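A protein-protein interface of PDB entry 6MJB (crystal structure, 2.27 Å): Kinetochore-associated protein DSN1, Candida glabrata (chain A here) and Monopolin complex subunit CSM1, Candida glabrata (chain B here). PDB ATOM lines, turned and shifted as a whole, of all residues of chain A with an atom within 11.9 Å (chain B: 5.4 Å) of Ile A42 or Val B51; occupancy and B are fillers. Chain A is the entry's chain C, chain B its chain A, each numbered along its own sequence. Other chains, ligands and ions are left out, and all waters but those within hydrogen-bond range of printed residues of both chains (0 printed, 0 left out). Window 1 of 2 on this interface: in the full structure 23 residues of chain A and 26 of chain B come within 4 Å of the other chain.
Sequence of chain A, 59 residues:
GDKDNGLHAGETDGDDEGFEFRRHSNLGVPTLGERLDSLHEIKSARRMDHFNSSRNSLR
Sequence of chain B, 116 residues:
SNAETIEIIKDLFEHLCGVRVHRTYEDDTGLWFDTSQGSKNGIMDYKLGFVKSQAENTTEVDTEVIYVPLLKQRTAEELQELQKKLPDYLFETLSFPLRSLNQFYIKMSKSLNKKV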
ATOM      1  N   ARG A  22       5.734 -26.771  19.793  1.00  0.00           N
ATOM      2  CA  ARG A  22       5.905 -25.336  19.793  1.00  0.00           C
ATOM      3  C   ARG A  22       4.733 -24.654  20.493  1.00  0.00           C
ATOM      4  O   ARG A  22       3.582 -25.103  20.406  1.00  0.00           O
ATOM      5  CB  ARG A  22       6.127 -24.818  18.384  1.00  0.00           C
ATOM      6  CG  ARG A  22       5.003 -24.946  17.452  1.00  0.00           C
ATOM      7  CD  ARG A  22       5.383 -24.233  16.178  1.00  0.00           C
ATOM      8  NE  ARG A  22       6.395 -24.964  15.422  1.00  0.00           N
ATOM      9  CZ  ARG A  22       7.135 -24.420  14.461  1.00  0.00           C
ATOM     10  NH1 ARG A  22       6.984 -23.133  14.163  1.00  0.00           N
ATOM     11  NH2 ARG A  22       8.032 -25.152  13.805  1.00  0.00           N
ATOM     12  N   HIS A  24       2.083 -21.635  21.433  1.00  0.00           N
ATOM     13  CA  HIS A  24       1.290 -20.669  20.693  1.00  0.00           C
ATOM     14  C   HIS A  24       0.441 -19.844  21.646  1.00  0.00           C
ATOM     15  O   HIS A  24       0.062 -20.287  22.730  1.00  0.00           O
ATOM     16  CB  HIS A  24       0.387 -21.337  19.651  1.00  0.00           C
ATOM     17  CG  HIS A  24       1.141 -22.079  18.602  1.00  0.00           C
ATOM     18  ND1 HIS A  24       1.151 -23.454  18.530  1.00  0.00           N
ATOM     19  CD2 HIS A  24       1.923 -21.643  17.589  1.00  0.00           C
ATOM     20  CE1 HIS A  24       1.904 -23.831  17.512  1.00  0.00           C
ATOM     21  NE2 HIS A  24       2.392 -22.750  16.932  1.00  0.00           N
ATOM     22  N   LEU A  27      -4.364 -16.525  20.036  1.00  0.00           N
ATOM     23  CA  LEU A  27      -4.828 -15.588  19.024  1.00  0.00           C
ATOM     24  C   LEU A  27      -5.848 -16.218  18.085  1.00  0.00           C
ATOM     25  O   LEU A  27      -6.619 -15.491  17.447  1.00  0.00           O
ATOM     26  CB  LEU A  27      -3.631 -15.044  18.237  1.00  0.00           C
ATOM     27  CG  LEU A  27      -3.836 -13.791  17.389  1.00  0.00           C
ATOM     28  CD1 LEU A  27      -4.137 -12.602  18.287  1.00  0.00           C
ATOM     29  CD2 LEU A  27      -2.623 -13.509  16.521  1.00  0.00           C
ATOM     30  N   GLY A  33      -7.220 -23.562   5.004  1.00  0.00           N
ATOM     31  CA  GLY A  33      -6.888 -22.681   3.899  1.00  0.00           C
ATOM     32  C   GLY A  33      -5.954 -21.556   4.304  1.00  0.00           C
ATOM     33  O   GLY A  33      -5.039 -21.198   3.558  1.00  0.00           O
ATOM     34  N   GLU A  34      -6.165 -20.988   5.492  1.00  0.00           N
ATOM     35  CA  GLU A  34      -5.309 -19.889   5.934  1.00  0.00           C
ATOM     36  C   GLU A  34      -3.870 -20.350   6.153  1.00  0.00           C
ATOM     37  O   GLU A  34      -2.931 -19.610   5.827  1.00  0.00           O
ATOM     38  CB  GLU A  34      -5.886 -19.261   7.205  1.00  0.00           C
ATOM     39  CG  GLU A  34      -7.140 -18.427   6.971  1.00  0.00           C
ATOM     40  CD  GLU A  34      -7.937 -18.157   8.263  1.00  0.00           C
ATOM     41  OE1 GLU A  34      -7.787 -18.922   9.247  1.00  0.00           O
ATOM     42  OE2 GLU A  34      -8.719 -17.176   8.298  1.00  0.00           O
ATOM     43  N   ARG A  35      -3.677 -21.566   6.688  1.00  0.00           N
ATOM     44  CA  ARG A  35      -2.335 -22.138   6.774  1.00  0.00           C
ATOM     45  C   ARG A  35      -1.678 -22.138   5.413  1.00  0.00           C
ATOM     46  O   ARG A  35      -0.527 -21.717   5.268  1.00  0.00           O
ATOM     47  CB  ARG A  35      -2.376 -23.573   7.306  1.00  0.00           C
ATOM     48  CG  ARG A  35      -2.919 -23.721   8.703  1.00  0.00           C
ATOM     49  CD  ARG A  35      -2.683 -25.129   9.245  1.00  0.00           C
ATOM     50  NE  ARG A  35      -3.405 -25.295  10.493  1.00  0.00           N
ATOM     51  CZ  ARG A  35      -2.935 -24.926  11.677  1.00  0.00           C
ATOM     52  NH1 ARG A  35      -1.728 -24.389  11.779  1.00  0.00           N
ATOM     53  NH2 ARG A  35      -3.683 -25.087  12.756  1.00  0.00           N
ATOM     54  N   LEU A  36      -2.407 -22.610   4.404  1.00  0.00           N
ATOM     55  CA  LEU A  36      -1.907 -22.590   3.036  1.00  0.00           C
ATOM     56  C   LEU A  36      -1.624 -21.165   2.581  1.00  0.00           C
ATOM     57  O   LEU A  36      -0.576 -20.887   1.990  1.00  0.00           O
ATOM     58  CB  LEU A  36      -2.922 -23.259   2.108  1.00  0.00           C
ATOM     59  CG  LEU A  36      -3.325 -24.699   2.429  1.00  0.00           C
ATOM     60  CD1 LEU A  36      -4.037 -25.322   1.230  1.00  0.00           C
ATOM     61  CD2 LEU A  36      -2.122 -25.547   2.866  1.00  0.00           C
ATOM     62  N   ASP A  37      -2.557 -20.251   2.842  1.00  0.00           N
ATOM     63  CA  ASP A  37      -2.391 -18.876   2.376  1.00  0.00           C
ATOM     64  C   ASP A  37      -1.119 -18.255   2.941  1.00  0.00           C
ATOM     65  O   ASP A  37      -0.363 -17.605   2.209  1.00  0.00           O
ATOM     66  CB  ASP A  37      -3.609 -18.033   2.747  1.00  0.00           C
ATOM     67  CG  ASP A  37      -4.851 -18.457   2.004  1.00  0.00           C
ATOM     68  OD1 ASP A  37      -4.713 -19.131   0.958  1.00  0.00           O
ATOM     69  OD2 ASP A  37      -5.965 -18.108   2.458  1.00  0.00           O
ATOM     70  N   SER A  38      -0.857 -18.464   4.237  1.00  0.00           N
ATOM     71  CA  SER A  38       0.314 -17.865   4.873  1.00  0.00           C
ATOM     72  C   SER A  38       1.595 -18.291   4.172  1.00  0.00           C
ATOM     73  O   SER A  38       2.442 -17.453   3.842  1.00  0.00           O
ATOM     74  CB  SER A  38       0.384 -18.240   6.363  1.00  0.00           C
ATOM     75  OG  SER A  38      -0.763 -17.832   7.085  1.00  0.00           O
ATOM     76  N   LEU A  39       1.770 -19.598   3.960  1.00  0.00           N
ATOM     77  CA  LEU A  39       2.971 -20.083   3.281  1.00  0.00           C
ATOM     78  C   LEU A  39       3.108 -19.455   1.899  1.00  0.00           C
ATOM     79  O   LEU A  39       4.195 -19.024   1.497  1.00  0.00           O
ATOM     80  CB  LEU A  39       2.940 -21.612   3.172  1.00  0.00           C
ATOM     81  CG  LEU A  39       3.219 -22.387   4.467  1.00  0.00           C
ATOM     82  CD1 LEU A  39       2.939 -23.883   4.311  1.00  0.00           C
ATOM     83  CD2 LEU A  39       4.642 -22.156   4.949  1.00  0.00           C
ATOM     84  N   HIS A  40       2.015 -19.415   1.144  1.00  0.00           N
ATOM     85  CA  HIS A  40       2.088 -18.833  -0.188  1.00  0.00           C
ATOM     86  C   HIS A  40       2.447 -17.346  -0.121  1.00  0.00           C
ATOM     87  O   HIS A  40       3.283 -16.865  -0.891  1.00  0.00           O
ATOM     88  CB  HIS A  40       0.764 -19.054  -0.923  1.00  0.00           C
ATOM     89  CG  HIS A  40       0.730 -18.434  -2.282  1.00  0.00           C
ATOM     90  ND1 HIS A  40       0.213 -17.179  -2.512  1.00  0.00           N
ATOM     91  CD2 HIS A  40       1.173 -18.885  -3.480  1.00  0.00           C
ATOM     92  CE1 HIS A  40       0.331 -16.885  -3.795  1.00  0.00           C
ATOM     93  NE2 HIS A  40       0.911 -17.903  -4.405  1.00  0.00           N
ATOM     94  N   GLU A  41       1.840 -16.608   0.812  1.00  0.00           N
ATOM     95  CA  GLU A  41       2.046 -15.161   0.872  1.00  0.00           C
ATOM     96  C   GLU A  41       3.471 -14.809   1.292  1.00  0.00           C
ATOM     97  O   GLU A  41       4.073 -13.876   0.744  1.00  0.00           O
ATOM     98  CB  GLU A  41       1.004 -14.538   1.803  1.00  0.00           C
ATOM     99  CG  GLU A  41      -0.378 -14.455   1.148  1.00  0.00           C
ATOM    100  CD  GLU A  41      -1.531 -14.645   2.132  1.00  0.00           C
ATOM    101  OE1 GLU A  41      -1.271 -14.727   3.357  1.00  0.00           O
ATOM    102  OE2 GLU A  41      -2.698 -14.724   1.675  1.00  0.00           O
ATOM    103  N   ILE A  42       4.038 -15.548   2.248  1.00  0.00           N
ATOM    104  CA  ILE A  42       5.453 -15.385   2.570  1.00  0.00           C
ATOM    105  C   ILE A  42       6.309 -15.640   1.339  1.00  0.00           C
ATOM    106  O   ILE A  42       7.194 -14.848   0.990  1.00  0.00           O
ATOM    107  CB  ILE A  42       5.854 -16.331   3.710  1.00  0.00           C
ATOM    108  CG1 ILE A  42       5.141 -15.944   5.003  1.00  0.00           C
ATOM    109  CG2 ILE A  42       7.375 -16.338   3.884  1.00  0.00           C
ATOM    110  CD1 ILE A  42       5.368 -16.932   6.122  1.00  0.00           C
ATOM    111  N   LYS A  43       6.061 -16.768   0.673  1.00  0.00           N
ATOM    112  CA  LYS A  43       6.893 -17.185  -0.446  1.00  0.00           C
ATOM    113  C   LYS A  43       6.857 -16.171  -1.579  1.00  0.00           C
ATOM    114  O   LYS A  43       7.887 -15.876  -2.190  1.00  0.00           O
ATOM    115  CB  LYS A  43       6.434 -18.560  -0.928  1.00  0.00           C
ATOM    116  CG  LYS A  43       6.991 -19.008  -2.260  1.00  0.00           C
ATOM    117  CD  LYS A  43       6.269 -20.282  -2.678  1.00  0.00           C
ATOM    118  CE  LYS A  43       6.710 -20.777  -4.034  1.00  0.00           C
ATOM    119  NZ  LYS A  43       6.168 -22.146  -4.279  1.00  0.00           N
ATOM    120  N   SER A  44       5.689 -15.621  -1.868  1.00  0.00           N
ATOM    121  CA  SER A  44       5.538 -14.698  -2.977  1.00  0.00           C
ATOM    122  C   SER A  44       5.697 -13.216  -2.588  1.00  0.00           C
ATOM    123  O   SER A  44       5.594 -12.359  -3.469  1.00  0.00           O
ATOM    124  CB  SER A  44       4.183 -14.912  -3.628  1.00  0.00           C
ATOM    125  OG  SER A  44       3.165 -14.614  -2.693  1.00  0.00           O
ATOM    126  N   ALA A  45       5.950 -12.890  -1.319  1.00  0.00           N
ATOM    127  CA  ALA A  45       6.005 -11.483  -0.910  1.00  0.00           C
ATOM    128  C   ALA A  45       7.199 -10.754  -1.526  1.00  0.00           C
ATOM    129  O   ALA A  45       8.314 -11.279  -1.593  1.00  0.00           O
ATOM    130  CB  ALA A  45       6.063 -11.348   0.618  1.00  0.00           C
ATOM    131  N   ARG A  46       6.957  -9.527  -1.973  1.00  0.00           N
ATOM    132  CA  ARG A  46       8.023  -8.669  -2.464  1.00  0.00           C
ATOM    133  C   ARG A  46       8.687  -7.972  -1.285  1.00  0.00           C
ATOM    134  O   ARG A  46       8.012  -7.321  -0.480  1.00  0.00           O
ATOM    135  CB  ARG A  46       7.484  -7.641  -3.449  1.00  0.00           C
ATOM    136  CG  ARG A  46       8.464  -6.523  -3.697  1.00  0.00           C
ATOM    137  CD  ARG A  46       7.876  -5.472  -4.570  1.00  0.00           C
ATOM    138  NE  ARG A  46       8.944  -4.675  -5.137  1.00  0.00           N
ATOM    139  CZ  ARG A  46       8.764  -3.662  -5.970  1.00  0.00           C
ATOM    140  NH1 ARG A  46       7.543  -3.308  -6.339  1.00  0.00           N
ATOM    141  NH2 ARG A  46       9.813  -3.013  -6.441  1.00  0.00           N
ATOM    142  N   ARG A  47      10.002  -8.096  -1.188  1.00  0.00           N
ATOM    143  CA  ARG A  47      10.731  -7.465  -0.097  1.00  0.00           C
ATOM    144  C   ARG A  47      10.847  -5.957  -0.321  1.00  0.00           C
ATOM    145  O   ARG A  47      11.176  -5.505  -1.421  1.00  0.00           O
ATOM    146  CB  ARG A  47      12.114  -8.091   0.027  1.00  0.00           C
ATOM    147  CG  ARG A  47      12.934  -7.518   1.145  1.00  0.00           C
ATOM    148  CD  ARG A  47      12.245  -7.719   2.468  1.00  0.00           C
ATOM    149  NE  ARG A  47      13.095  -7.308   3.579  1.00  0.00           N
ATOM    150  CZ  ARG A  47      12.872  -7.642   4.848  1.00  0.00           C
ATOM    151  NH1 ARG A  47      11.822  -8.399   5.164  1.00  0.00           N
ATOM    152  NH2 ARG A  47      13.702  -7.222   5.801  1.00  0.00           N
ATOM    153  N   MET A  48      10.549  -5.184   0.722  1.00  0.00           N
ATOM    154  CA  MET A  48      10.722  -3.736   0.739  1.00  0.00           C
ATOM    155  C   MET A  48      11.268  -3.347   2.103  1.00  0.00           C
ATOM    156  O   MET A  48      10.807  -3.868   3.120  1.00  0.00           O
ATOM    157  CB  MET A  48       9.405  -3.001   0.504  1.00  0.00           C
ATOM    158  CG  MET A  48       9.038  -2.778  -0.928  1.00  0.00           C
ATOM    159  SD  MET A  48       7.757  -1.513  -0.975  1.00  0.00           S
ATOM    160  CE  MET A  48       8.738  -0.025  -0.833  1.00  0.00           C
ATOM    161  N   THR B  29       3.552 -20.353  10.956  1.00  0.00           N
ATOM    162  CA  THR B  29       4.464 -19.342  10.440  1.00  0.00           C
ATOM    163  C   THR B  29       4.523 -18.111  11.336  1.00  0.00           C
ATOM    164  O   THR B  29       5.583 -17.491  11.455  1.00  0.00           O
ATOM    165  CB  THR B  29       4.074 -18.913   9.022  1.00  0.00           C
ATOM    166  OG1 THR B  29       2.885 -18.124   9.064  1.00  0.00           O
ATOM    167  CG2 THR B  29       3.861 -20.119   8.119  1.00  0.00           C
ATOM    168  N   GLY B  30       3.408 -17.741  11.968  1.00  0.00           N
ATOM    169  CA  GLY B  30       3.387 -16.576  12.829  1.00  0.00           C
ATOM    170  C   GLY B  30       2.006 -16.095  13.237  1.00  0.00           C
ATOM    171  O   GLY B  30       1.041 -16.870  13.274  1.00  0.00           O
ATOM    172  N   LEU B  31       1.914 -14.806  13.568  1.00  0.00           N
ATOM    173  CA  LEU B  31       0.683 -14.162  13.999  1.00  0.00           C
ATOM    174  C   LEU B  31       0.096 -13.388  12.824  1.00  0.00           C
ATOM    175  O   LEU B  31       0.835 -12.756  12.060  1.00  0.00           O
ATOM    176  CB  LEU B  31       0.955 -13.225  15.185  1.00  0.00           C
ATOM    177  CG  LEU B  31       1.829 -13.811  16.296  1.00  0.00           C
ATOM    178  CD1 LEU B  31       2.153 -12.791  17.372  1.00  0.00           C
ATOM    179  CD2 LEU B  31       1.167 -15.009  16.919  1.00  0.00           C
ATOM    180  N   TRP B  32      -1.230 -13.443  12.669  1.00  0.00           N
ATOM    181  CA  TRP B  32      -1.888 -12.877  11.495  1.00  0.00           C
ATOM    182  C   TRP B  32      -3.130 -12.081  11.899  1.00  0.00           C
ATOM    183  O   TRP B  32      -3.836 -12.435  12.847  1.00  0.00           O
ATOM    184  CB  TRP B  32      -2.235 -13.996  10.468  1.00  0.00           C
ATOM    185  CG  TRP B  32      -0.978 -14.645   9.874  1.00  0.00           C
ATOM    186  CD1 TRP B  32      -0.213 -15.644  10.436  1.00  0.00           C
ATOM    187  CD2 TRP B  32      -0.340 -14.316   8.631  1.00  0.00           C
ATOM    188  NE1 TRP B  32       0.849 -15.950   9.617  1.00  0.00           N
ATOM    189  CE2 TRP B  32       0.798 -15.148   8.508  1.00  0.00           C
ATOM    190  CE3 TRP B  32      -0.621 -13.404   7.608  1.00  0.00           C
ATOM    191  CZ2 TRP B  32       1.648 -15.093   7.406  1.00  0.00           C
ATOM    192  CZ3 TRP B  32       0.235 -13.348   6.509  1.00  0.00           C
ATOM    193  CH2 TRP B  32       1.350 -14.192   6.418  1.00  0.00           C
ATOM    194  N   GLY B  49       0.882 -10.138   8.619  1.00  0.00           N
ATOM    195  CA  GLY B  49       1.480 -11.299   9.267  1.00  0.00           C
ATOM    196  C   GLY B  49       2.856 -10.993   9.833  1.00  0.00           C
ATOM    197  O   GLY B  49       3.672 -10.352   9.176  1.00  0.00           O
ATOM    198  N   PHE B  50       3.108 -11.475  11.052  1.00  0.00           N
ATOM    199  CA  PHE B  50       4.364 -11.237  11.761  1.00  0.00           C
ATOM    200  C   PHE B  50       5.091 -12.563  11.899  1.00  0.00           C
ATOM    201  O   PHE B  50       4.669 -13.426  12.668  1.00  0.00           O
ATOM    202  CB  PHE B  50       4.110 -10.601  13.130  1.00  0.00           C
ATOM    203  CG  PHE B  50       3.402  -9.279  13.055  1.00  0.00           C
ATOM    204  CD1 PHE B  50       2.044  -9.207  12.762  1.00  0.00           C
ATOM    205  CD2 PHE B  50       4.095  -8.101  13.253  1.00  0.00           C
ATOM    206  CE1 PHE B  50       1.398  -7.983  12.681  1.00  0.00           C
ATOM    207  CE2 PHE B  50       3.451  -6.879  13.180  1.00  0.00           C
ATOM    208  CZ  PHE B  50       2.109  -6.819  12.898  1.00  0.00           C
ATOM    209  N   VAL B  51       6.177 -12.738  11.157  1.00  0.00           N
ATOM    210  CA  VAL B  51       6.908 -13.999  11.148  1.00  0.00           C
ATOM    211  C   VAL B  51       8.284 -13.735  11.739  1.00  0.00           C
ATOM    212  O   VAL B  51       9.025 -12.871  11.255  1.00  0.00           O
ATOM    213  CB  VAL B  51       6.984 -14.603   9.738  1.00  0.00           C
ATOM    214  CG1 VAL B  51       5.581 -14.899   9.235  1.00  0.00           C
ATOM    215  CG2 VAL B  51       7.664 -13.653   8.785  1.00  0.00           C
ATOM    216  N   LYS B  52       8.606 -14.447  12.812  1.00  0.00           N
ATOM    217  CA  LYS B  52       9.845 -14.239  13.545  1.00  0.00           C
ATOM    218  C   LYS B  52      10.893 -15.214  13.037  1.00  0.00           C
ATOM    219  O   LYS B  52      10.594 -16.386  12.793  1.00  0.00           O
ATOM    220  CB  LYS B  52       9.643 -14.428  15.052  1.00  0.00           C
ATOM    221  N   SER B  53      12.112 -14.713  12.850  1.00  0.00           N
ATOM    222  CA  SER B  53      13.262 -15.555  12.510  1.00  0.00           C
ATOM    223  C   SER B  53      14.467 -15.150  13.353  1.00  0.00           C
ATOM    224  O   SER B  53      14.503 -14.043  13.897  1.00  0.00           O
ATOM    225  CB  SER B  53      13.606 -15.455  11.021  1.00  0.00           C
ATOM    226  OG  SER B  53      14.087 -14.166  10.691  1.00  0.00           O
ATOM    227  N   ASP B  62      14.791 -11.738  14.643  1.00  0.00           N
ATOM    228  CA  ASP B  62      14.215 -10.601  13.938  1.00  0.00           C
ATOM    229  C   ASP B  62      12.783 -10.912  13.511  1.00  0.00           C
ATOM    230  O   ASP B  62      12.427 -12.067  13.262  1.00  0.00           O
ATOM    231  CB  ASP B  62      15.057 -10.238  12.713  1.00  0.00           C
ATOM    232  N   THR B  63      11.964  -9.870  13.419  1.00  0.00           N
ATOM    233  CA  THR B  63      10.553 -10.005  13.073  1.00  0.00           C
ATOM    234  C   THR B  63      10.290  -9.384  11.708  1.00  0.00           C
ATOM    235  O   THR B  63      10.618  -8.217  11.472  1.00  0.00           O
ATOM    236  CB  THR B  63       9.673  -9.351  14.137  1.00  0.00           C
ATOM    237  OG1 THR B  63       9.665 -10.177  15.307  1.00  0.00           O
ATOM    238  CG2 THR B  63       8.234  -9.156  13.623  1.00  0.00           C
ATOM    239  N   GLU B  64       9.692 -10.164  10.818  1.00  0.00           N
ATOM    240  CA  GLU B  64       9.275  -9.678   9.513  1.00  0.00           C
ATOM    241  C   GLU B  64       7.763  -9.523   9.479  1.00  0.00           C
ATOM    242  O   GLU B  64       7.030 -10.277  10.129  1.00  0.00           O
ATOM    243  CB  GLU B  64       9.724 -10.619   8.395  1.00  0.00           C
ATOM    244  CG  GLU B  64      11.236 -10.728   8.279  1.00  0.00           C
ATOM    245  CD  GLU B  64      11.910  -9.365   8.224  1.00  0.00           C
ATOM    246  OE1 GLU B  64      11.494  -8.531   7.388  1.00  0.00           O
ATOM    247  OE2 GLU B  64      12.840  -9.116   9.025  1.00  0.00           O
ATOM    248  N   VAL B  65       7.308  -8.531   8.722  1.00  0.00           N
ATOM    249  CA  VAL B  65       5.888  -8.268   8.520  1.00  0.00           C
ATOM    250  C   VAL B  65       5.556  -8.602   7.076  1.00  0.00           C
ATOM    251  O   VAL B  65       6.273  -8.187   6.159  1.00  0.00           O
ATOM    252  CB  VAL B  65       5.526  -6.806   8.840  1.00  0.00           C
ATOM    253  CG1 VAL B  65       4.027  -6.603   8.736  1.00  0.00           C
ATOM    254  CG2 VAL B  65       6.006  -6.442  10.221  1.00  0.00           C
ATOM    255  N   ILE B  66       4.488  -9.361   6.875  1.00  0.00           N
ATOM    256  CA  ILE B  66       3.965  -9.646   5.547  1.00  0.00           C
ATOM    257  C   ILE B  66       2.645  -8.900   5.401  1.00  0.00           C
ATOM    258  O   ILE B  66       1.758  -9.008   6.256  1.00  0.00           O
ATOM    259  CB  ILE B  66       3.801 -11.157   5.289  1.00  0.00           C
ATOM    260  CG1 ILE B  66       5.150 -11.782   4.913  1.00  0.00           C
ATOM    261  CG2 ILE B  66       2.874 -11.407   4.104  1.00  0.00           C
ATOM    262  CD1 ILE B  66       5.999 -12.119   6.061  1.00  0.00           C
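Of the 19 printed residues of chain A, 6 touch a printed residue of chain B.
Of the 14 printed residues of chain B, 5 touch a printed residue of chain A.
Hydrophobic or aromatic side chains of chain B that line the printed part of chain A: Leu B31, Trp B32 and Val B51.
Among the printed residues, pairs that only touch across the chains: Ser A38 with Trp B32 (3.4 Å), Ser A38 with Thr B29 (3.7 Å), Ile A42 with Val B51 (3.7 Å), Ile A42 with Thr B29 (3.7 Å), Glu A41 with Trp B32 (3.8 Å), Leu A27 with Leu B31 (3.8 Å) and Leu A39 with Thr B29 (3.8 Å).
Of chain B, only Thr B29 and Val B51 come within 4 Å of Ile A42.
Thr B29 touches three residues of chain A.
No residue of chain A comes within 4 Å of Gly B30.
No residue of chain A comes within 4 Å of Gly B49.
No residue of chain A comes within 4 Å of Phe B50.
Lys B52 touches none of the printed residues of chain A.
No residue of chain A comes within 4 Å of Ser B53.
Asp B62 touches none of the printed residues of chain A.
No residue of chain A comes within 4 Å of Thr B63.
Glu B64 touches one residue of chain A.
No residue of chain A comes within 4 Å of Ile B66.
Printed residues of chain B within 4 Å of Glu A41: Trp B32.
Of the printed residues of chain A, Trp B32 touches Ser A38 (3.4 Å) and Glu A41 (3.8 Å).
His A40 touches none of the printed residues of chain B.
The indole nitrogen (NE1) of Trp B32 is in hydrogen-bond range of the side-chain hydroxyl (OG1) of Thr B29, 3.0 Å away.
N of Phe B50 sits at hydrogen-bond distance from O of Leu B31.
The backbone NH (N) of Val B51 sits at hydrogen-bond distance from the backbone carbonyl oxygen (O) of Glu B64.
O of Glu A34 sits at hydrogen-bond distance from OG of Ser A38 (3.1 Å).
The guanidinium group (NH2) of Arg A47 is in salt-bridge range of the side-chain carboxylate (OE1) of Glu B64.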
